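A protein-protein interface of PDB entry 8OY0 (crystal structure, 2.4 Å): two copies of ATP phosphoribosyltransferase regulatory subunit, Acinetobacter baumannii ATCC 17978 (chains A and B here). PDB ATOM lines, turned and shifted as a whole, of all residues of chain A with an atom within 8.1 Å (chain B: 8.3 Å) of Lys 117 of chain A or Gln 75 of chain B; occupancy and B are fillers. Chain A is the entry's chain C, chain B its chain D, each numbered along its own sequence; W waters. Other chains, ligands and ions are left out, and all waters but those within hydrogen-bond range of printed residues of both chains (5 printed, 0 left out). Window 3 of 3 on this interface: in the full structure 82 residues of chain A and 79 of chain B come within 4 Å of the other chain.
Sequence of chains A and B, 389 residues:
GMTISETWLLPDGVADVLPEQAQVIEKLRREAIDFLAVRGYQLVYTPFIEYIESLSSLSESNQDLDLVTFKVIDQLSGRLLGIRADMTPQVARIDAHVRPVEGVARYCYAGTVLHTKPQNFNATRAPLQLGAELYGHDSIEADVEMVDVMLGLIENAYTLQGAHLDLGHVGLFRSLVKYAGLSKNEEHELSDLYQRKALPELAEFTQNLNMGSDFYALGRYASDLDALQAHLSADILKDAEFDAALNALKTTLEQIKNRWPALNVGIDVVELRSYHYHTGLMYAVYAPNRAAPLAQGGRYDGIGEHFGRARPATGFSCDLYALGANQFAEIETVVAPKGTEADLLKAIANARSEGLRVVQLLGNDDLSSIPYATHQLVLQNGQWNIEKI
Water W5 lies within hydrogen-bond range of the side-chain carboxylate (OD2) of Asp 74 of chain B (2.4 Å), the side-chain hydroxyl (OH) of Tyr 51 of chain B (2.7 Å), the backbone NH (N) of Asp 12 of chain A (2.9 Å) and the guanidinium group (NH2) of Arg 125 of chain A (3.5 Å).
Water W2 lies within hydrogen-bond range of the side-chain amide oxygen (OE1) of Gln 75 of chain B (2.6 Å) and the side-chain amino group (NZ) of Lys 117 of chain A (3.1 Å).
Water W1 lies within hydrogen-bond range of the backbone carbonyl oxygen (O) of Leu 67 of chain A (2.6 Å) and the side-chain amide nitrogen (NE2) of Gln 75 of chain B (2.8 Å).
Water W3 bridges the backbone NH of Gln 75 of chain B (2.8 Å) and the backbone carbonyl oxygen of Thr 116 of chain A (3.3 Å).
Water W4 bridges OH of Tyr 51 of chain B (3.0 Å) and OD1 of Asp 12 of chain A (3.3 Å).
O of Asp 12 of chain A lies within hydrogen-bond range of NE of Arg 125 of chain A (2.7 Å).
The backbone carbonyl oxygen of Gly 13 of chain A sits at hydrogen-bond distance from the backbone NH of Arg 125 of chain A (2.7 Å).
O of Val 68 of chain A lies within hydrogen-bond range of N of Thr 116 of chain A, at 2.8 Å.
The side-chain amide oxygen of Gln 119 of chain A sits close to the backbone carbonyl oxygen of Lys 117 of chain A, 3.0 Å away.
The backbone carbonyl oxygen (O) of Val 72 of chain B lies within hydrogen-bond range of the backbone NH (N) of Leu 81 of chain B (2.6 Å).
The side-chain carboxylate (OD1) of Asp 74 of chain B lies close to the backbone NH (N) of Leu 76 of chain B (3.2 Å).
No position is printed for both chains.
Of the 9 pairs that touch across the chains among the printed residues, none has its exchanged pair printed and touching as well.
Of the 21 printed residues of chain A, 6 touch a printed residue of chain B.
Printed residues of chain A that touch a printed residue of chain B: Asp 12, Phe 70, Lys 71, Thr 116, Lys 117 and Arg 125.
Hydrophobic or aromatic side chains of chain A within 4 Å of the printed part of chain B: Phe 70.
Hydrophobic or aromatic side chains of chain B that line the printed part of chain A: Val 72, Leu 76 and Leu 81.
Along chain B the printed residues that touch a printed residue of chain A span positions 72 to 81.
Among the printed residues, 9 pairs touch across the chains.
The side-chain carboxylate (OD1) of Asp 74 of chain B is in salt-bridge range of the guanidinium group (NH1) of Arg 125 of chain A.
Among the printed residues, merely in contact across the chains: Asp 12 of chain A with Leu 76 of chain B (3.8 Å), Phe 70 of chain A with Val 72 of chain B (3.8 Å), Phe 70 of chain A with Leu 81 of chain B (3.96 Å), Lys 71 of chain A with Val 72 of chain B (3.4 Å), Thr 116 of chain A with Gln 75 of chain B (3.6 Å), Lys 117 of chain A with Gln 75 of chain B (3.99 Å), Lys 117 of chain A with Leu 76 of chain B (3.97 Å) and Arg 125 of chain A with Leu 76 of chain B (3.6 Å).
Of the printed residues of chain B, Lys 117 of chain A touches Gln 75 and Leu 76.
Printed residues of chain A within 4 Å of Gln 75 of chain B: Thr 116 and Lys 117.
Of chain B, only Gln 75 (3.6 Å) comes within 4 Å of Thr 116 of chain A.
Of the printed residues of chain A, Asp 74 of chain B touches Arg 125.
Of the printed residues of chain B, Asp 12 of chain A touches Leu 76.
Of the printed residues of chain A, Leu 76 of chain B touches Asp 12 (3.8 Å), Lys 117 (3.97 Å) and Arg 125 (3.6 Å).
Printed residues of chain B within 4 Å of Phe 70 of chain A: Val 72 (3.8 Å) and Leu 81 (3.96 Å).
Leu 114 of chain A touches none of the printed residues of chain B.
Ser 77 of chain B touches none of the printed residues of chain A.
The nearest printed residue of chain A that does not touch Gln 75 of chain B is Leu 67 of chain A (4.6 Å).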
ATOM      1  N   ASP A  12      23.372 -15.478  20.188  1.00  0.00           N
ATOM      2  CA  ASP A  12      23.550 -16.586  19.269  1.00  0.00           C
ATOM      3  C   ASP A  12      22.609 -17.724  19.642  1.00  0.00           C
ATOM      4  O   ASP A  12      22.437 -18.027  20.827  1.00  0.00           O
ATOM      5  CB  ASP A  12      24.989 -17.095  19.279  1.00  0.00           C
ATOM      6  CG  ASP A  12      25.939 -16.201  18.509  1.00  0.00           C
ATOM      7  OD1 ASP A  12      25.495 -15.121  18.076  1.00  0.00           O
ATOM      8  OD2 ASP A  12      27.108 -16.606  18.323  1.00  0.00           O
ATOM      9  N   GLY A  13      22.017 -18.337  18.610  1.00  0.00           N
ATOM     10  CA  GLY A  13      21.153 -19.497  18.771  1.00  0.00           C
ATOM     11  C   GLY A  13      19.731 -19.118  19.177  1.00  0.00           C
ATOM     12  O   GLY A  13      18.932 -19.987  19.498  1.00  0.00           O
ATOM     13  N   ASP A  66      23.502 -30.597  34.817  1.00  0.00           N
ATOM     14  CA  ASP A  66      24.612 -30.754  33.835  1.00  0.00           C
ATOM     15  C   ASP A  66      24.877 -29.393  33.186  1.00  0.00           C
ATOM     16  O   ASP A  66      24.268 -28.410  33.584  1.00  0.00           O
ATOM     17  CB  ASP A  66      24.304 -31.896  32.859  1.00  0.00           C
ATOM     18  CG  ASP A  66      23.158 -31.625  31.892  1.00  0.00           C
ATOM     19  OD1 ASP A  66      22.187 -30.954  32.319  1.00  0.00           O
ATOM     20  OD2 ASP A  66      23.211 -32.146  30.736  1.00  0.00           O
ATOM     21  N   LEU A  67      25.783 -29.342  32.212  1.00  0.00           N
ATOM     22  CA  LEU A  67      26.250 -28.075  31.673  1.00  0.00           C
ATOM     23  C   LEU A  67      25.161 -27.353  30.889  1.00  0.00           C
ATOM     24  O   LEU A  67      25.239 -26.135  30.744  1.00  0.00           O
ATOM     25  CB  LEU A  67      27.469 -28.328  30.777  1.00  0.00           C
ATOM     26  CG  LEU A  67      28.737 -28.766  31.501  1.00  0.00           C
ATOM     27  CD1 LEU A  67      29.906 -28.820  30.537  1.00  0.00           C
ATOM     28  CD2 LEU A  67      29.048 -27.834  32.669  1.00  0.00           C
ATOM     29  N   VAL A  68      24.159 -28.091  30.399  1.00  0.00           N
ATOM     30  CA  VAL A  68      23.258 -27.564  29.383  1.00  0.00           C
ATOM     31  C   VAL A  68      22.212 -26.634  30.002  1.00  0.00           C
ATOM     32  O   VAL A  68      21.642 -25.806  29.300  1.00  0.00           O
ATOM     33  CB  VAL A  68      22.583 -28.697  28.580  1.00  0.00           C
ATOM     34  CG1 VAL A  68      23.608 -29.655  27.982  1.00  0.00           C
ATOM     35  CG2 VAL A  68      21.582 -29.471  29.422  1.00  0.00           C
ATOM     36  N   THR A  69      21.958 -26.791  31.306  1.00  0.00           N
ATOM     37  CA  THR A  69      20.906 -26.067  32.010  1.00  0.00           C
ATOM     38  C   THR A  69      21.366 -24.671  32.432  1.00  0.00           C
ATOM     39  O   THR A  69      22.366 -24.539  33.130  1.00  0.00           O
ATOM     40  CB  THR A  69      20.452 -26.881  33.225  1.00  0.00           C
ATOM     41  OG1 THR A  69      19.747 -28.010  32.726  1.00  0.00           O
ATOM     42  CG2 THR A  69      19.510 -26.142  34.137  1.00  0.00           C
ATOM     43  N   PHE A  70      20.613 -23.638  32.021  1.00  0.00           N
ATOM     44  CA  PHE A  70      20.795 -22.289  32.543  1.00  0.00           C
ATOM     45  C   PHE A  70      20.482 -22.278  34.039  1.00  0.00           C
ATOM     46  O   PHE A  70      19.504 -22.886  34.463  1.00  0.00           O
ATOM     47  CB  PHE A  70      19.905 -21.275  31.817  1.00  0.00           C
ATOM     48  CG  PHE A  70      20.425 -20.771  30.493  1.00  0.00           C
ATOM     49  CD1 PHE A  70      21.435 -19.822  30.441  1.00  0.00           C
ATOM     50  CD2 PHE A  70      19.899 -21.239  29.293  1.00  0.00           C
ATOM     51  CE1 PHE A  70      21.908 -19.355  29.225  1.00  0.00           C
ATOM     52  CE2 PHE A  70      20.381 -20.773  28.077  1.00  0.00           C
ATOM     53  CZ  PHE A  70      21.382 -19.833  28.047  1.00  0.00           C
ATOM     54  N   LYS A  71      21.311 -21.586  34.830  1.00  0.00           N
ATOM     55  CA  LYS A  71      21.186 -21.602  36.280  1.00  0.00           C
ATOM     56  C   LYS A  71      21.041 -20.174  36.807  1.00  0.00           C
ATOM     57  O   LYS A  71      21.766 -19.287  36.364  1.00  0.00           O
ATOM     58  CB  LYS A  71      22.402 -22.300  36.890  1.00  0.00           C
ATOM     59  CG  LYS A  71      22.481 -23.799  36.610  1.00  0.00           C
ATOM     60  CD  LYS A  71      23.801 -24.403  37.013  1.00  0.00           C
ATOM     61  CE  LYS A  71      23.877 -25.889  36.750  1.00  0.00           C
ATOM     62  NZ  LYS A  71      23.887 -26.150  35.299  1.00  0.00           N
ATOM     63  N   LEU A 114      15.458 -24.481  27.039  1.00  0.00           N
ATOM     64  CA  LEU A 114      16.641 -23.671  26.799  1.00  0.00           C
ATOM     65  C   LEU A 114      17.894 -24.487  27.083  1.00  0.00           C
ATOM     66  O   LEU A 114      17.936 -25.251  28.040  1.00  0.00           O
ATOM     67  CB  LEU A 114      16.594 -22.425  27.687  1.00  0.00           C
ATOM     68  CG  LEU A 114      15.568 -21.360  27.308  1.00  0.00           C
ATOM     69  CD1 LEU A 114      15.830 -20.081  28.084  1.00  0.00           C
ATOM     70  CD2 LEU A 114      15.591 -21.067  25.826  1.00  0.00           C
ATOM     71  N   HIS A 115      18.908 -24.284  26.237  1.00  0.00           N
ATOM     72  CA  HIS A 115      20.208 -24.917  26.371  1.00  0.00           C
ATOM     73  C   HIS A 115      21.276 -23.830  26.372  1.00  0.00           C
ATOM     74  O   HIS A 115      21.208 -22.901  25.583  1.00  0.00           O
ATOM     75  CB  HIS A 115      20.419 -25.928  25.236  1.00  0.00           C
ATOM     76  CG  HIS A 115      19.338 -26.950  25.134  1.00  0.00           C
ATOM     77  ND1 HIS A 115      18.934 -27.510  23.939  1.00  0.00           N
ATOM     78  CD2 HIS A 115      18.622 -27.556  26.093  1.00  0.00           C
ATOM     79  CE1 HIS A 115      17.981 -28.407  24.182  1.00  0.00           C
ATOM     80  NE2 HIS A 115      17.776 -28.445  25.487  1.00  0.00           N
ATOM     81  N   THR A 116      22.256 -23.949  27.270  1.00  0.00           N
ATOM     82  CA  THR A 116      23.294 -22.939  27.407  1.00  0.00           C
ATOM     83  C   THR A 116      24.122 -22.849  26.129  1.00  0.00           C
ATOM     84  O   THR A 116      24.647 -21.787  25.811  1.00  0.00           O
ATOM     85  CB  THR A 116      24.187 -23.232  28.614  1.00  0.00           C
ATOM     86  OG1 THR A 116      24.565 -24.602  28.517  1.00  0.00           O
ATOM     87  CG2 THR A 116      23.490 -22.968  29.933  1.00  0.00           C
ATOM     88  N   LYS A 117      24.256 -23.986  25.438  1.00  0.00           N
ATOM     89  CA  LYS A 117      24.829 -24.059  24.104  1.00  0.00           C
ATOM     90  C   LYS A 117      23.984 -25.004  23.253  1.00  0.00           C
ATOM     91  O   LYS A 117      23.411 -25.953  23.780  1.00  0.00           O
ATOM     92  CB  LYS A 117      26.280 -24.543  24.173  1.00  0.00           C
ATOM     93  CG  LYS A 117      27.257 -23.515  24.721  1.00  0.00           C
ATOM     94  CD  LYS A 117      28.595 -24.079  25.106  1.00  0.00           C
ATOM     95  CE  LYS A 117      29.533 -22.992  25.570  1.00  0.00           C
ATOM     96  NZ  LYS A 117      30.850 -23.555  25.937  1.00  0.00           N
ATOM     97  N   PRO A 118      23.881 -24.779  21.921  1.00  0.00           N
ATOM     98  CA  PRO A 118      23.126 -25.673  21.040  1.00  0.00           C
ATOM     99  C   PRO A 118      23.529 -27.135  21.193  1.00  0.00           C
ATOM    100  O   PRO A 118      24.707 -27.445  21.299  1.00  0.00           O
ATOM    101  CB  PRO A 118      23.470 -25.180  19.628  1.00  0.00           C
ATOM    102  CG  PRO A 118      23.841 -23.727  19.818  1.00  0.00           C
ATOM    103  CD  PRO A 118      24.491 -23.661  21.186  1.00  0.00           C
ATOM    104  N   GLN A 119      22.531 -28.021  21.227  1.00  0.00           N
ATOM    105  CA  GLN A 119      22.730 -29.455  21.335  1.00  0.00           C
ATOM    106  C   GLN A 119      22.370 -30.085  19.990  1.00  0.00           C
ATOM    107  O   GLN A 119      21.622 -29.495  19.217  1.00  0.00           O
ATOM    108  CB  GLN A 119      21.845 -30.002  22.461  1.00  0.00           C
ATOM    109  CG  GLN A 119      22.003 -29.287  23.795  1.00  0.00           C
ATOM    110  CD  GLN A 119      23.313 -29.613  24.468  1.00  0.00           C
ATOM    111  OE1 GLN A 119      24.144 -28.749  24.733  1.00  0.00           O
ATOM    112  NE2 GLN A 119      23.516 -30.884  24.753  1.00  0.00           N
ATOM    113  N   ASN A 120      22.906 -31.279  19.707  1.00  0.00           N
ATOM    114  CA  ASN A 120      22.411 -32.111  18.613  1.00  0.00           C
ATOM    115  C   ASN A 120      22.452 -31.366  17.277  1.00  0.00           C
ATOM    116  O   ASN A 120      21.508 -31.458  16.498  1.00  0.00           O
ATOM    117  CB  ASN A 120      20.970 -32.576  18.865  1.00  0.00           C
ATOM    118  CG  ASN A 120      20.766 -33.163  20.247  1.00  0.00           C
ATOM    119  OD1 ASN A 120      21.721 -33.594  20.894  1.00  0.00           O
ATOM    120  ND2 ASN A 120      19.526 -33.185  20.713  1.00  0.00           N
ATOM    121  N   ASN A 122      21.885 -28.568  16.465  1.00  0.00           N
ATOM    122  CA  ASN A 122      20.724 -27.710  16.331  1.00  0.00           C
ATOM    123  C   ASN A 122      21.221 -26.287  16.088  1.00  0.00           C
ATOM    124  O   ASN A 122      22.286 -25.914  16.571  1.00  0.00           O
ATOM    125  CB  ASN A 122      19.842 -27.820  17.580  1.00  0.00           C
ATOM    126  CG  ASN A 122      18.382 -27.544  17.307  1.00  0.00           C
ATOM    127  OD1 ASN A 122      18.054 -26.541  16.677  1.00  0.00           O
ATOM    128  ND2 ASN A 122      17.507 -28.430  17.756  1.00  0.00           N
ATOM    129  N   ALA A 123      20.455 -25.499  15.328  1.00  0.00           N
ATOM    130  CA  ALA A 123      20.767 -24.087  15.151  1.00  0.00           C
ATOM    131  C   ALA A 123      20.433 -23.312  16.427  1.00  0.00           C
ATOM    132  O   ALA A 123      21.127 -22.353  16.761  1.00  0.00           O
ATOM    133  CB  ALA A 123      20.025 -23.524  13.958  1.00  0.00           C
ATOM    134  N   THR A 124      19.389 -23.752  17.149  1.00  0.00           N
ATOM    135  CA  THR A 124      18.773 -22.941  18.187  1.00  0.00           C
ATOM    136  C   THR A 124      19.155 -23.448  19.579  1.00  0.00           C
ATOM    137  O   THR A 124      19.254 -24.649  19.829  1.00  0.00           O
ATOM    138  CB  THR A 124      17.251 -22.845  17.985  1.00  0.00           C
ATOM    139  OG1 THR A 124      16.692 -22.000  18.992  1.00  0.00           O
ATOM    140  CG2 THR A 124      16.536 -24.175  18.050  1.00  0.00           C
ATOM    141  N   ARG A 125      19.347 -22.488  20.492  1.00  0.00           N
ATOM    142  CA  ARG A 125      19.458 -22.766  21.914  1.00  0.00           C
ATOM    143  C   ARG A 125      18.074 -22.832  22.548  1.00  0.00           C
ATOM    144  O   ARG A 125      17.983 -22.978  23.757  1.00  0.00           O
ATOM    145  CB  ARG A 125      20.282 -21.683  22.619  1.00  0.00           C
ATOM    146  CG  ARG A 125      21.770 -21.746  22.313  1.00  0.00           C
ATOM    147  CD  ARG A 125      22.605 -20.950  23.295  1.00  0.00           C
ATOM    148  NE  ARG A 125      22.639 -19.516  23.046  1.00  0.00           N
ATOM    149  CZ  ARG A 125      23.323 -18.650  23.782  1.00  0.00           C
ATOM    150  NH1 ARG A 125      23.829 -19.024  24.942  1.00  0.00           N
ATOM    151  NH2 ARG A 125      23.468 -17.405  23.361  1.00  0.00           N
ATOM    152  N   ALA A 126      17.012 -22.727  21.733  1.00  0.00           N
ATOM    153  CA  ALA A 126      15.658 -22.630  22.255  1.00  0.00           C
ATOM    154  C   ALA A 126      14.711 -23.492  21.429  1.00  0.00           C
ATOM    155  O   ALA A 126      13.744 -22.985  20.856  1.00  0.00           O
ATOM    156  CB  ALA A 126      15.218 -21.181  22.278  1.00  0.00           C
ATOM    157  N   PRO A 127      14.930 -24.822  21.357  1.00  0.00           N
ATOM    158  CA  PRO A 127      14.061 -25.688  20.565  1.00  0.00           C
ATOM    159  C   PRO A 127      12.669 -25.779  21.179  1.00  0.00           C
ATOM    160  O   PRO A 127      12.504 -25.588  22.382  1.00  0.00           O
ATOM    161  CB  PRO A 127      14.781 -27.048  20.566  1.00  0.00           C
ATOM    162  CG  PRO A 127      15.680 -27.021  21.793  1.00  0.00           C
ATOM    163  CD  PRO A 127      16.019 -25.561  22.015  1.00  0.00           C
ATOM    164  N   TYR B  51      19.626 -10.408  25.416  1.00  0.00           N
ATOM    165  CA  TYR B  51      20.564  -9.562  26.129  1.00  0.00           C
ATOM    166  C   TYR B  51      19.770  -8.620  27.030  1.00  0.00           C
ATOM    167  O   TYR B  51      18.705  -8.149  26.658  1.00  0.00           O
ATOM    168  CB  TYR B  51      21.446  -8.805  25.139  1.00  0.00           C
ATOM    169  CG  TYR B  51      22.408  -9.660  24.353  1.00  0.00           C
ATOM    170  CD1 TYR B  51      23.261 -10.548  24.989  1.00  0.00           C
ATOM    171  CD2 TYR B  51      22.482  -9.574  22.973  1.00  0.00           C
ATOM    172  CE1 TYR B  51      24.154 -11.330  24.273  1.00  0.00           C
ATOM    173  CE2 TYR B  51      23.373 -10.342  22.245  1.00  0.00           C
ATOM    174  CZ  TYR B  51      24.214 -11.223  22.896  1.00  0.00           C
ATOM    175  OH  TYR B  51      25.079 -11.996  22.168  1.00  0.00           O
ATOM    176  N   VAL B  72      21.005 -14.153  33.707  1.00  0.00           N
ATOM    177  CA  VAL B  72      21.987 -15.215  33.539  1.00  0.00           C
ATOM    178  C   VAL B  72      23.053 -14.754  32.554  1.00  0.00           C
ATOM    179  O   VAL B  72      22.775 -13.969  31.654  1.00  0.00           O
ATOM    180  CB  VAL B  72      21.370 -16.526  33.009  1.00  0.00           C
ATOM    181  CG1 VAL B  72      20.451 -17.154  34.020  1.00  0.00           C
ATOM    182  CG2 VAL B  72      20.636 -16.346  31.690  1.00  0.00           C
ATOM    183  N   ILE B  73      24.247 -15.336  32.685  1.00  0.00           N
ATOM    184  CA  ILE B  73      25.371 -15.042  31.819  1.00  0.00           C
ATOM    185  C   ILE B  73      25.279 -15.902  30.560  1.00  0.00           C
ATOM    186  O   ILE B  73      24.942 -17.085  30.622  1.00  0.00           O
ATOM    187  CB  ILE B  73      26.682 -15.250  32.611  1.00  0.00           C
ATOM    188  CG1 ILE B  73      27.753 -14.223  32.236  1.00  0.00           C
ATOM    189  CG2 ILE B  73      27.175 -16.691  32.548  1.00  0.00           C
ATOM    190  CD1 ILE B  73      27.462 -12.834  32.786  1.00  0.00           C
ATOM    191  N   ASP B  74      25.538 -15.263  29.418  1.00  0.00           N
ATOM    192  CA  ASP B  74      25.679 -15.934  28.134  1.00  0.00           C
ATOM    193  C   ASP B  74      27.116 -16.416  27.989  1.00  0.00           C
ATOM    194  O   ASP B  74      28.029 -15.607  27.931  1.00  0.00           O
ATOM    195  CB  ASP B  74      25.344 -14.980  26.984  1.00  0.00           C
ATOM    196  CG  ASP B  74      25.356 -15.607  25.610  1.00  0.00           C
ATOM    197  OD1 ASP B  74      25.331 -16.854  25.536  1.00  0.00           O
ATOM    198  OD2 ASP B  74      25.433 -14.834  24.624  1.00  0.00           O
ATOM    199  N   GLN B  75      27.301 -17.736  27.923  1.00  0.00           N
ATOM    200  CA  GLN B  75      28.628 -18.322  27.825  1.00  0.00           C
ATOM    201  C   GLN B  75      29.248 -18.007  26.463  1.00  0.00           C
ATOM    202  O   GLN B  75      30.460 -17.855  26.363  1.00  0.00           O
ATOM    203  CB  GLN B  75      28.546 -19.823  28.103  1.00  0.00           C
ATOM    204  CG  GLN B  75      28.269 -20.116  29.568  1.00  0.00           C
ATOM    205  CD  GLN B  75      27.987 -21.573  29.833  1.00  0.00           C
ATOM    206  OE1 GLN B  75      28.751 -22.447  29.445  1.00  0.00           O
ATOM    207  NE2 GLN B  75      26.876 -21.846  30.494  1.00  0.00           N
ATOM    208  N   LEU B  76      28.414 -17.851  25.428  1.00  0.00           N
ATOM    209  CA  LEU B  76      28.908 -17.562  24.089  1.00  0.00           C
ATOM    210  C   LEU B  76      29.451 -16.134  23.964  1.00  0.00           C
ATOM    211  O   LEU B  76      30.429 -15.940  23.257  1.00  0.00           O
ATOM    212  CB  LEU B  76      27.789 -17.850  23.078  1.00  0.00           C
ATOM    213  CG  LEU B  76      27.326 -19.311  23.028  1.00  0.00           C
ATOM    214  CD1 LEU B  76      26.293 -19.544  21.939  1.00  0.00           C
ATOM    215  CD2 LEU B  76      28.511 -20.250  22.836  1.00  0.00           C
ATOM    216  N   SER B  77      28.853 -15.134  24.626  1.00  0.00           N
ATOM    217  CA  SER B  77      29.280 -13.744  24.468  1.00  0.00           C
ATOM    218  C   SER B  77      29.942 -13.176  25.727  1.00  0.00           C
ATOM    219  O   SER B  77      30.703 -12.215  25.644  1.00  0.00           O
ATOM    220  CB  SER B  77      28.117 -12.881  24.083  1.00  0.00           C
ATOM    221  OG  SER B  77      27.137 -12.877  25.104  1.00  0.00           O
ATOM    222  N   GLY B  78      29.598 -13.710  26.901  1.00  0.00           N
ATOM    223  CA  GLY B  78      30.041 -13.140  28.164  1.00  0.00           C
ATOM    224  C   GLY B  78      29.126 -12.011  28.643  1.00  0.00           C
ATOM    225  O   GLY B  78      29.383 -11.392  29.677  1.00  0.00           O
ATOM    226  N   ARG B  79      28.059 -11.744  27.878  1.00  0.00           N
ATOM    227  CA  ARG B  79      27.113 -10.687  28.197  1.00  0.00           C
ATOM    228  C   ARG B  79      26.000 -11.256  29.064  1.00  0.00           C
ATOM    229  O   ARG B  79      25.760 -12.458  29.076  1.00  0.00           O
ATOM    230  CB  ARG B  79      26.515 -10.077  26.926  1.00  0.00           C
ATOM    231  CG  ARG B  79      27.515  -9.276  26.106  1.00  0.00           C
ATOM    232  CD  ARG B  79      26.942  -8.716  24.820  1.00  0.00           C
ATOM    233  NE  ARG B  79      25.827  -7.820  25.089  1.00  0.00           N
ATOM    234  CZ  ARG B  79      25.095  -7.208  24.163  1.00  0.00           C
ATOM    235  NH1 ARG B  79      25.404  -7.329  22.884  1.00  0.00           N
ATOM    236  NH2 ARG B  79      24.060  -6.467  24.524  1.00  0.00           N
ATOM    237  N   LEU B  80      25.300 -10.357  29.757  1.00  0.00           N
ATOM    238  CA  LEU B  80      24.220 -10.746  30.638  1.00  0.00           C
ATOM    239  C   LEU B  80      22.934 -10.884  29.832  1.00  0.00           C
ATOM    240  O   LEU B  80      22.606 -10.015  29.025  1.00  0.00           O
ATOM    241  CB  LEU B  80      24.100  -9.684  31.731  1.00  0.00           C
ATOM    242  CG  LEU B  80      23.429 -10.137  33.024  1.00  0.00           C
ATOM    243  CD1 LEU B  80      24.287 -11.161  33.750  1.00  0.00           C
ATOM    244  CD2 LEU B  80      23.177  -8.939  33.921  1.00  0.00           C
ATOM    245  N   LEU B  81      22.230 -12.003  30.044  1.00  0.00           N
ATOM    246  CA  LEU B  81      20.925 -12.227  29.451  1.00  0.00           C
ATOM    247  C   LEU B  81      19.846 -11.951  30.493  1.00  0.00           C
ATOM    248  O   LEU B  81      20.102 -11.965  31.686  1.00  0.00           O
ATOM    249  CB  LEU B  81      20.812 -13.688  28.988  1.00  0.00           C
ATOM    250  CG  LEU B  81      21.819 -14.165  27.948  1.00  0.00           C
ATOM    251  CD1 LEU B  81      21.723 -15.673  27.770  1.00  0.00           C
ATOM    252  CD2 LEU B  81      21.605 -13.461  26.616  1.00  0.00           C
HETATM  253  O   HOH W   1      26.655 -24.215  31.886  1.00  0.00           O
HETATM  254  O   HOH W   2      31.144 -21.978  28.581  1.00  0.00           O
HETATM  255  O   HOH W   3      25.192 -19.597  28.183  1.00  0.00           O
HETATM  256  O   HOH W   4      24.565 -12.177  19.174  1.00  0.00           O
HETATM  257  O   HOH W   5      25.334 -14.699  22.184  1.00  0.00           O
